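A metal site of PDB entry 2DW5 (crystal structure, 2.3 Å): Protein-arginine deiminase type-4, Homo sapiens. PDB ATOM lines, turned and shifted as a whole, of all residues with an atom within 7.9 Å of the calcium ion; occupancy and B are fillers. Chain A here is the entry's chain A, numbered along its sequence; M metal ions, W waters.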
ATOM      1  N   ASP A 358      19.245  34.193  19.291  1.00  0.00           N
ATOM      2  CA  ASP A 358      18.913  33.191  18.298  1.00  0.00           C
ATOM      3  C   ASP A 358      20.041  32.253  17.815  1.00  0.00           C
ATOM      4  O   ASP A 358      19.734  31.129  17.393  1.00  0.00           O
ATOM      5  CB  ASP A 358      18.227  33.915  17.125  1.00  0.00           C
ATOM      6  CG  ASP A 358      16.803  34.402  17.464  1.00  0.00           C
ATOM      7  OD1 ASP A 358      16.147  33.849  18.396  1.00  0.00           O
ATOM      8  OD2 ASP A 358      16.329  35.319  16.770  1.00  0.00           O
ATOM      9  N   GLU A 359      21.317  32.674  17.854  1.00  0.00           N
ATOM     10  CA  GLU A 359      22.402  31.766  17.439  1.00  0.00           C
ATOM     11  C   GLU A 359      22.801  30.817  18.526  1.00  0.00           C
ATOM     12  O   GLU A 359      23.483  29.841  18.254  1.00  0.00           O
ATOM     13  CB  GLU A 359      23.714  32.488  17.048  1.00  0.00           C
ATOM     14  CG  GLU A 359      23.771  32.985  15.661  1.00  0.00           C
ATOM     15  CD  GLU A 359      24.038  31.967  14.615  1.00  0.00           C
ATOM     16  OE1 GLU A 359      24.630  30.919  14.880  1.00  0.00           O
ATOM     17  OE2 GLU A 359      23.691  32.280  13.465  1.00  0.00           O
ATOM     18  N   MET A 360      22.476  31.126  19.771  1.00  0.00           N
ATOM     19  CA  MET A 360      23.045  30.327  20.850  1.00  0.00           C
ATOM     20  C   MET A 360      22.133  30.176  22.077  1.00  0.00           C
ATOM     21  O   MET A 360      21.250  30.992  22.327  1.00  0.00           O
ATOM     22  CB  MET A 360      24.377  30.913  21.257  1.00  0.00           C
ATOM     23  CG  MET A 360      24.255  32.072  22.187  1.00  0.00           C
ATOM     24  SD  MET A 360      25.853  32.766  22.623  1.00  0.00           S
ATOM     25  CE  MET A 360      25.375  33.760  24.053  1.00  0.00           C
ATOM     26  N   PHE A 376      25.343  25.962  23.440  1.00  0.00           N
ATOM     27  CA  PHE A 376      24.818  25.245  22.323  1.00  0.00           C
ATOM     28  C   PHE A 376      24.664  26.262  21.196  1.00  0.00           C
ATOM     29  O   PHE A 376      23.827  27.166  21.251  1.00  0.00           O
ATOM     30  CB  PHE A 376      23.511  24.578  22.720  1.00  0.00           C
ATOM     31  CG  PHE A 376      22.932  23.689  21.689  1.00  0.00           C
ATOM     32  CD1 PHE A 376      23.706  23.081  20.732  1.00  0.00           C
ATOM     33  CD2 PHE A 376      21.555  23.424  21.700  1.00  0.00           C
ATOM     34  CE1 PHE A 376      23.123  22.237  19.781  1.00  0.00           C
ATOM     35  CE2 PHE A 376      20.975  22.563  20.780  1.00  0.00           C
ATOM     36  CZ  PHE A 376      21.744  21.968  19.825  1.00  0.00           C
ATOM     37  N   ASP A 377      25.473  26.090  20.184  1.00  0.00           N
ATOM     38  CA  ASP A 377      25.514  26.991  19.067  1.00  0.00           C
ATOM     39  C   ASP A 377      24.571  26.506  17.973  1.00  0.00           C
ATOM     40  O   ASP A 377      24.739  25.385  17.439  1.00  0.00           O
ATOM     41  CB  ASP A 377      26.966  27.030  18.566  1.00  0.00           C
ATOM     42  CG  ASP A 377      27.164  27.887  17.344  1.00  0.00           C
ATOM     43  OD1 ASP A 377      26.213  28.627  16.932  1.00  0.00           O
ATOM     44  OD2 ASP A 377      28.291  27.806  16.791  1.00  0.00           O
ATOM     45  N   SER A 378      23.580  27.331  17.635  1.00  0.00           N
ATOM     46  CA  SER A 378      22.555  26.972  16.663  1.00  0.00           C
ATOM     47  C   SER A 378      23.107  27.040  15.237  1.00  0.00           C
ATOM     48  O   SER A 378      23.822  27.966  14.919  1.00  0.00           O
ATOM     49  CB  SER A 378      21.375  27.963  16.738  1.00  0.00           C
ATOM     50  OG  SER A 378      20.479  27.862  15.639  1.00  0.00           O
ATOM     51  N   PRO A 379      22.671  26.124  14.365  1.00  0.00           N
ATOM     52  CA  PRO A 379      23.083  26.128  12.964  1.00  0.00           C
ATOM     53  C   PRO A 379      22.589  27.310  12.103  1.00  0.00           C
ATOM     54  O   PRO A 379      22.989  27.433  10.951  1.00  0.00           O
ATOM     55  CB  PRO A 379      22.468  24.842  12.417  1.00  0.00           C
ATOM     56  CG  PRO A 379      21.257  24.622  13.271  1.00  0.00           C
ATOM     57  CD  PRO A 379      21.688  25.067  14.657  1.00  0.00           C
ATOM     58  N   ARG A 380      21.717  28.176  12.629  1.00  0.00           N
ATOM     59  CA  ARG A 380      21.206  29.266  11.802  1.00  0.00           C
ATOM     60  C   ARG A 380      22.310  30.089  11.146  1.00  0.00           C
ATOM     61  O   ARG A 380      22.098  30.646  10.067  1.00  0.00           O
ATOM     62  CB  ARG A 380      20.205  30.147  12.544  1.00  0.00           C
ATOM     63  CG  ARG A 380      20.757  31.178  13.474  1.00  0.00           C
ATOM     64  CD  ARG A 380      19.879  32.428  13.479  1.00  0.00           C
ATOM     65  NE  ARG A 380      20.550  33.456  14.272  1.00  0.00           N
ATOM     66  CZ  ARG A 380      20.410  34.765  14.154  1.00  0.00           C
ATOM     67  NH1 ARG A 380      19.594  35.323  13.284  1.00  0.00           N
ATOM     68  NH2 ARG A 380      21.114  35.539  14.961  1.00  0.00           N
ATOM     69  N   ASN A 381      23.484  30.153  11.786  1.00  0.00           N
ATOM     70  CA  ASN A 381      24.702  30.686  11.130  1.00  0.00           C
ATOM     71  C   ASN A 381      24.462  31.983  10.340  1.00  0.00           C
ATOM     72  O   ASN A 381      24.813  32.127   9.157  1.00  0.00           O
ATOM     73  CB  ASN A 381      25.339  29.607  10.258  1.00  0.00           C
ATOM     74  CG  ASN A 381      25.850  28.456  11.091  1.00  0.00           C
ATOM     75  OD1 ASN A 381      25.918  28.553  12.317  1.00  0.00           O
ATOM     76  ND2 ASN A 381      26.204  27.356  10.438  1.00  0.00           N
ATOM     77  N   ARG A 382      23.869  32.926  11.045  1.00  0.00           N
ATOM     78  CA  ARG A 382      23.656  34.270  10.550  1.00  0.00           C
ATOM     79  C   ARG A 382      24.922  35.102  10.888  1.00  0.00           C
ATOM     80  O   ARG A 382      26.012  34.542  11.062  1.00  0.00           O
ATOM     81  CB  ARG A 382      22.392  34.805  11.219  1.00  0.00           C
ATOM     82  CG  ARG A 382      21.499  35.564  10.309  1.00  0.00           C
ATOM     83  CD  ARG A 382      20.569  34.672   9.513  1.00  0.00           C
ATOM     84  NE  ARG A 382      19.220  34.576  10.074  1.00  0.00           N
ATOM     85  CZ  ARG A 382      18.349  35.578  10.245  1.00  0.00           C
ATOM     86  NH1 ARG A 382      18.661  36.840   9.965  1.00  0.00           N
ATOM     87  NH2 ARG A 382      17.156  35.321  10.725  1.00  0.00           N
ATOM     88  N   LEU A 384      25.958  36.493  13.555  1.00  0.00           N
ATOM     89  CA  LEU A 384      26.523  36.054  14.840  1.00  0.00           C
ATOM     90  C   LEU A 384      27.191  34.690  14.775  1.00  0.00           C
ATOM     91  O   LEU A 384      27.579  34.167  15.816  1.00  0.00           O
ATOM     92  CB  LEU A 384      25.469  36.048  15.953  1.00  0.00           C
ATOM     93  CG  LEU A 384      25.382  37.179  17.009  1.00  0.00           C
ATOM     94  CD1 LEU A 384      26.467  38.249  16.855  1.00  0.00           C
ATOM     95  CD2 LEU A 384      23.946  37.754  17.054  1.00  0.00           C
ATOM     96  N   LYS A 385      27.343  34.105  13.583  1.00  0.00           N
ATOM     97  CA  LYS A 385      27.872  32.731  13.454  1.00  0.00           C
ATOM     98  C   LYS A 385      29.125  32.460  14.285  1.00  0.00           C
ATOM     99  O   LYS A 385      29.295  31.363  14.816  1.00  0.00           O
ATOM    100  CB  LYS A 385      28.160  32.381  11.982  1.00  0.00           C
ATOM    101  N   GLU A 386      30.008  33.459  14.413  1.00  0.00           N
ATOM    102  CA  GLU A 386      31.314  33.263  15.047  1.00  0.00           C
ATOM    103  C   GLU A 386      31.315  33.485  16.553  1.00  0.00           C
ATOM    104  O   GLU A 386      32.187  32.934  17.244  1.00  0.00           O
ATOM    105  CB  GLU A 386      32.357  34.172  14.361  1.00  0.00           C
ATOM    106  CG  GLU A 386      32.689  33.743  12.946  1.00  0.00           C
ATOM    107  CD  GLU A 386      33.113  32.269  12.886  1.00  0.00           C
ATOM    108  OE1 GLU A 386      32.498  31.488  12.122  1.00  0.00           O
ATOM    109  OE2 GLU A 386      34.049  31.884  13.623  1.00  0.00           O
ATOM    110  N   PHE A 387      30.353  34.258  17.052  1.00  0.00           N
ATOM    111  CA  PHE A 387      30.325  34.690  18.463  1.00  0.00           C
ATOM    112  C   PHE A 387      30.435  33.574  19.492  1.00  0.00           C
ATOM    113  O   PHE A 387      31.179  33.717  20.478  1.00  0.00           O
ATOM    114  CB  PHE A 387      29.067  35.524  18.779  1.00  0.00           C
ATOM    115  CG  PHE A 387      29.069  36.139  20.153  1.00  0.00           C
ATOM    116  CD1 PHE A 387      29.943  37.172  20.460  1.00  0.00           C
ATOM    117  CD2 PHE A 387      28.198  35.688  21.141  1.00  0.00           C
ATOM    118  CE1 PHE A 387      29.967  37.751  21.719  1.00  0.00           C
ATOM    119  CE2 PHE A 387      28.205  36.268  22.414  1.00  0.00           C
ATOM    120  CZ  PHE A 387      29.100  37.303  22.698  1.00  0.00           C
ATOM    121  N   PRO A 388      29.676  32.463  19.281  1.00  0.00           N
ATOM    122  CA  PRO A 388      29.827  31.342  20.190  1.00  0.00           C
ATOM    123  C   PRO A 388      31.212  30.692  20.074  1.00  0.00           C
ATOM    124  O   PRO A 388      31.776  30.254  21.091  1.00  0.00           O
ATOM    125  CB  PRO A 388      28.734  30.358  19.737  1.00  0.00           C
ATOM    126  CG  PRO A 388      27.811  31.155  18.868  1.00  0.00           C
ATOM    127  CD  PRO A 388      28.709  32.172  18.218  1.00  0.00           C
ATOM    128  N   ILE A 389      31.753  30.662  18.859  1.00  0.00           N
ATOM    129  CA  ILE A 389      33.061  30.053  18.621  1.00  0.00           C
ATOM    130  C   ILE A 389      34.197  30.942  19.140  1.00  0.00           C
ATOM    131  O   ILE A 389      35.037  30.478  19.921  1.00  0.00           O
ATOM    132  CB  ILE A 389      33.284  29.710  17.140  1.00  0.00           C
ATOM    133  CG1 ILE A 389      32.253  28.691  16.661  1.00  0.00           C
ATOM    134  CG2 ILE A 389      34.720  29.179  16.932  1.00  0.00           C
ATOM    135  CD1 ILE A 389      32.275  28.440  15.148  1.00  0.00           C
ATOM    136  N   TYR A 399      31.586  24.126  24.360  1.00  0.00           N
ATOM    137  CA  TYR A 399      30.951  24.322  23.098  1.00  0.00           C
ATOM    138  C   TYR A 399      30.294  23.019  22.571  1.00  0.00           C
ATOM    139  O   TYR A 399      30.757  21.926  22.860  1.00  0.00           O
ATOM    140  CB  TYR A 399      32.014  24.829  22.133  1.00  0.00           C
ATOM    141  CG  TYR A 399      31.431  25.097  20.802  1.00  0.00           C
ATOM    142  CD1 TYR A 399      30.902  26.324  20.505  1.00  0.00           C
ATOM    143  CD2 TYR A 399      31.337  24.070  19.843  1.00  0.00           C
ATOM    144  CE1 TYR A 399      30.334  26.572  19.303  1.00  0.00           C
ATOM    145  CE2 TYR A 399      30.745  24.309  18.627  1.00  0.00           C
ATOM    146  CZ  TYR A 399      30.257  25.565  18.360  1.00  0.00           C
ATOM    147  OH  TYR A 399      29.713  25.839  17.132  1.00  0.00           O
ATOM    148  N   VAL A 400      29.229  23.184  21.785  1.00  0.00           N
ATOM    149  CA  VAL A 400      28.548  22.097  21.098  1.00  0.00           C
ATOM    150  C   VAL A 400      27.705  22.743  20.041  1.00  0.00           C
ATOM    151  O   VAL A 400      27.137  23.837  20.244  1.00  0.00           O
ATOM    152  CB  VAL A 400      27.450  21.341  21.974  1.00  0.00           C
ATOM    153  CG1 VAL A 400      27.100  19.889  21.366  1.00  0.00           C
ATOM    154  CG2 VAL A 400      27.829  21.324  23.457  1.00  0.00           C
ATOM    155  N   THR A 401      27.537  22.011  18.943  1.00  0.00           N
ATOM    156  CA  THR A 401      26.687  22.445  17.846  1.00  0.00           C
ATOM    157  C   THR A 401      26.076  21.201  17.185  1.00  0.00           C
ATOM    158  O   THR A 401      26.631  20.118  17.234  1.00  0.00           O
ATOM    159  CB  THR A 401      27.493  23.275  16.828  1.00  0.00           C
ATOM    160  OG1 THR A 401      26.580  24.038  16.047  1.00  0.00           O
ATOM    161  CG2 THR A 401      28.330  22.376  15.913  1.00  0.00           C
ATOM    162  N   ARG A 402      24.899  21.381  16.601  1.00  0.00           N
ATOM    163  CA  ARG A 402      24.218  20.339  15.845  1.00  0.00           C
ATOM    164  C   ARG A 402      23.656  20.930  14.559  1.00  0.00           C
ATOM    165  O   ARG A 402      23.582  22.155  14.393  1.00  0.00           O
ATOM    166  CB  ARG A 402      23.103  19.694  16.674  1.00  0.00           C
ATOM    167  CG  ARG A 402      23.590  18.762  17.778  1.00  0.00           C
ATOM    168  CD  ARG A 402      24.473  17.703  17.156  1.00  0.00           C
ATOM    169  NE  ARG A 402      24.814  16.619  18.059  1.00  0.00           N
ATOM    170  CZ  ARG A 402      25.917  16.549  18.787  1.00  0.00           C
ATOM    171  NH1 ARG A 402      26.806  17.532  18.774  1.00  0.00           N
ATOM    172  NH2 ARG A 402      26.115  15.481  19.550  1.00  0.00           N
ATOM    173  N   GLN A 405      25.429  22.777   8.543  1.00  0.00           N
ATOM    174  CA  GLN A 405      26.049  24.079   8.737  1.00  0.00           C
ATOM    175  C   GLN A 405      26.152  24.942   7.455  1.00  0.00           C
ATOM    176  O   GLN A 405      26.420  26.123   7.571  1.00  0.00           O
ATOM    177  CB  GLN A 405      27.425  23.900   9.402  1.00  0.00           C
ATOM    178  CG  GLN A 405      27.331  23.204  10.817  1.00  0.00           C
ATOM    179  CD  GLN A 405      26.756  24.139  11.889  1.00  0.00           C
ATOM    180  OE1 GLN A 405      26.875  25.364  11.789  1.00  0.00           O
ATOM    181  NE2 GLN A 405      26.138  23.556  12.901  1.00  0.00           N
ATOM    182  N   PHE A 415      17.249  29.935  18.376  1.00  0.00           N
ATOM    183  CA  PHE A 415      17.126  29.460  19.746  1.00  0.00           C
ATOM    184  C   PHE A 415      16.274  30.337  20.599  1.00  0.00           C
ATOM    185  O   PHE A 415      16.116  30.078  21.769  1.00  0.00           O
ATOM    186  CB  PHE A 415      18.504  29.203  20.354  1.00  0.00           C
ATOM    187  CG  PHE A 415      19.161  27.909  19.862  1.00  0.00           C
ATOM    188  CD1 PHE A 415      20.428  27.571  20.285  1.00  0.00           C
ATOM    189  CD2 PHE A 415      18.513  27.051  18.966  1.00  0.00           C
ATOM    190  CE1 PHE A 415      21.047  26.408  19.868  1.00  0.00           C
ATOM    191  CE2 PHE A 415      19.126  25.880  18.521  1.00  0.00           C
ATOM    192  CZ  PHE A 415      20.389  25.567  18.995  1.00  0.00           C
HETATM  193 CA    CA M   1      25.926  28.817  14.629  1.00  0.00          CA
HETATM  194  O   HOH W   1      26.734  26.487  14.314  1.00  0.00           O
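Four residues have an atom within 4 Å of the calcium ion: Glu 359, Asp 377, Ser 378 and Asn 381.
OD2 of Asp 377 lies within hydrogen-bond range of OH of Tyr 399 (2.5 Å).
The side-chain carboxylate (OE2) of Glu 359 lies within salt-bridge range of the guanidinium group (NE) of Arg 380 (3.4 Å).
The side-chain amide nitrogen of Asn 381 is in hydrogen-bond range of the side-chain amide oxygen of Gln 405 (2.5 Å).
The backbone NH (N) of Asp 377 is in hydrogen-bond range of the backbone carbonyl oxygen (O) of Val 400 (2.8 Å).
The backbone carbonyl oxygen (O) of Pro 379 sits close to the side-chain amide nitrogen (ND2) of Asn 381, 3.3 Å away.
The side-chain hydroxyl (OG) of Ser 378 lies close to the backbone NH (N) of Arg 380, at 3.3 Å.
The side-chain carboxylate (OE2) of Glu 359 sits at hydrogen-bond distance from the backbone NH (N) of Arg 382 (2.5 Å).
O of Asp 377 is in hydrogen-bond range of OG1 of Thr 401.
The calcium ion is bound by the backbone carbonyl oxygen (O) of Ser 378, the side-chain amide oxygen (OD1) of Asn 381, the side-chain carboxylate (OD1) of Asp 377, the side-chain carboxylate (OE1) of Glu 359 and water W1.
Water W1 lies within hydrogen-bond range of the side-chain amide oxygen of Gln 405 (2.8 Å), the side-chain hydroxyl of Thr 401 (3.0 Å) and the side-chain carboxylate of Asp 377 (3.2 Å).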
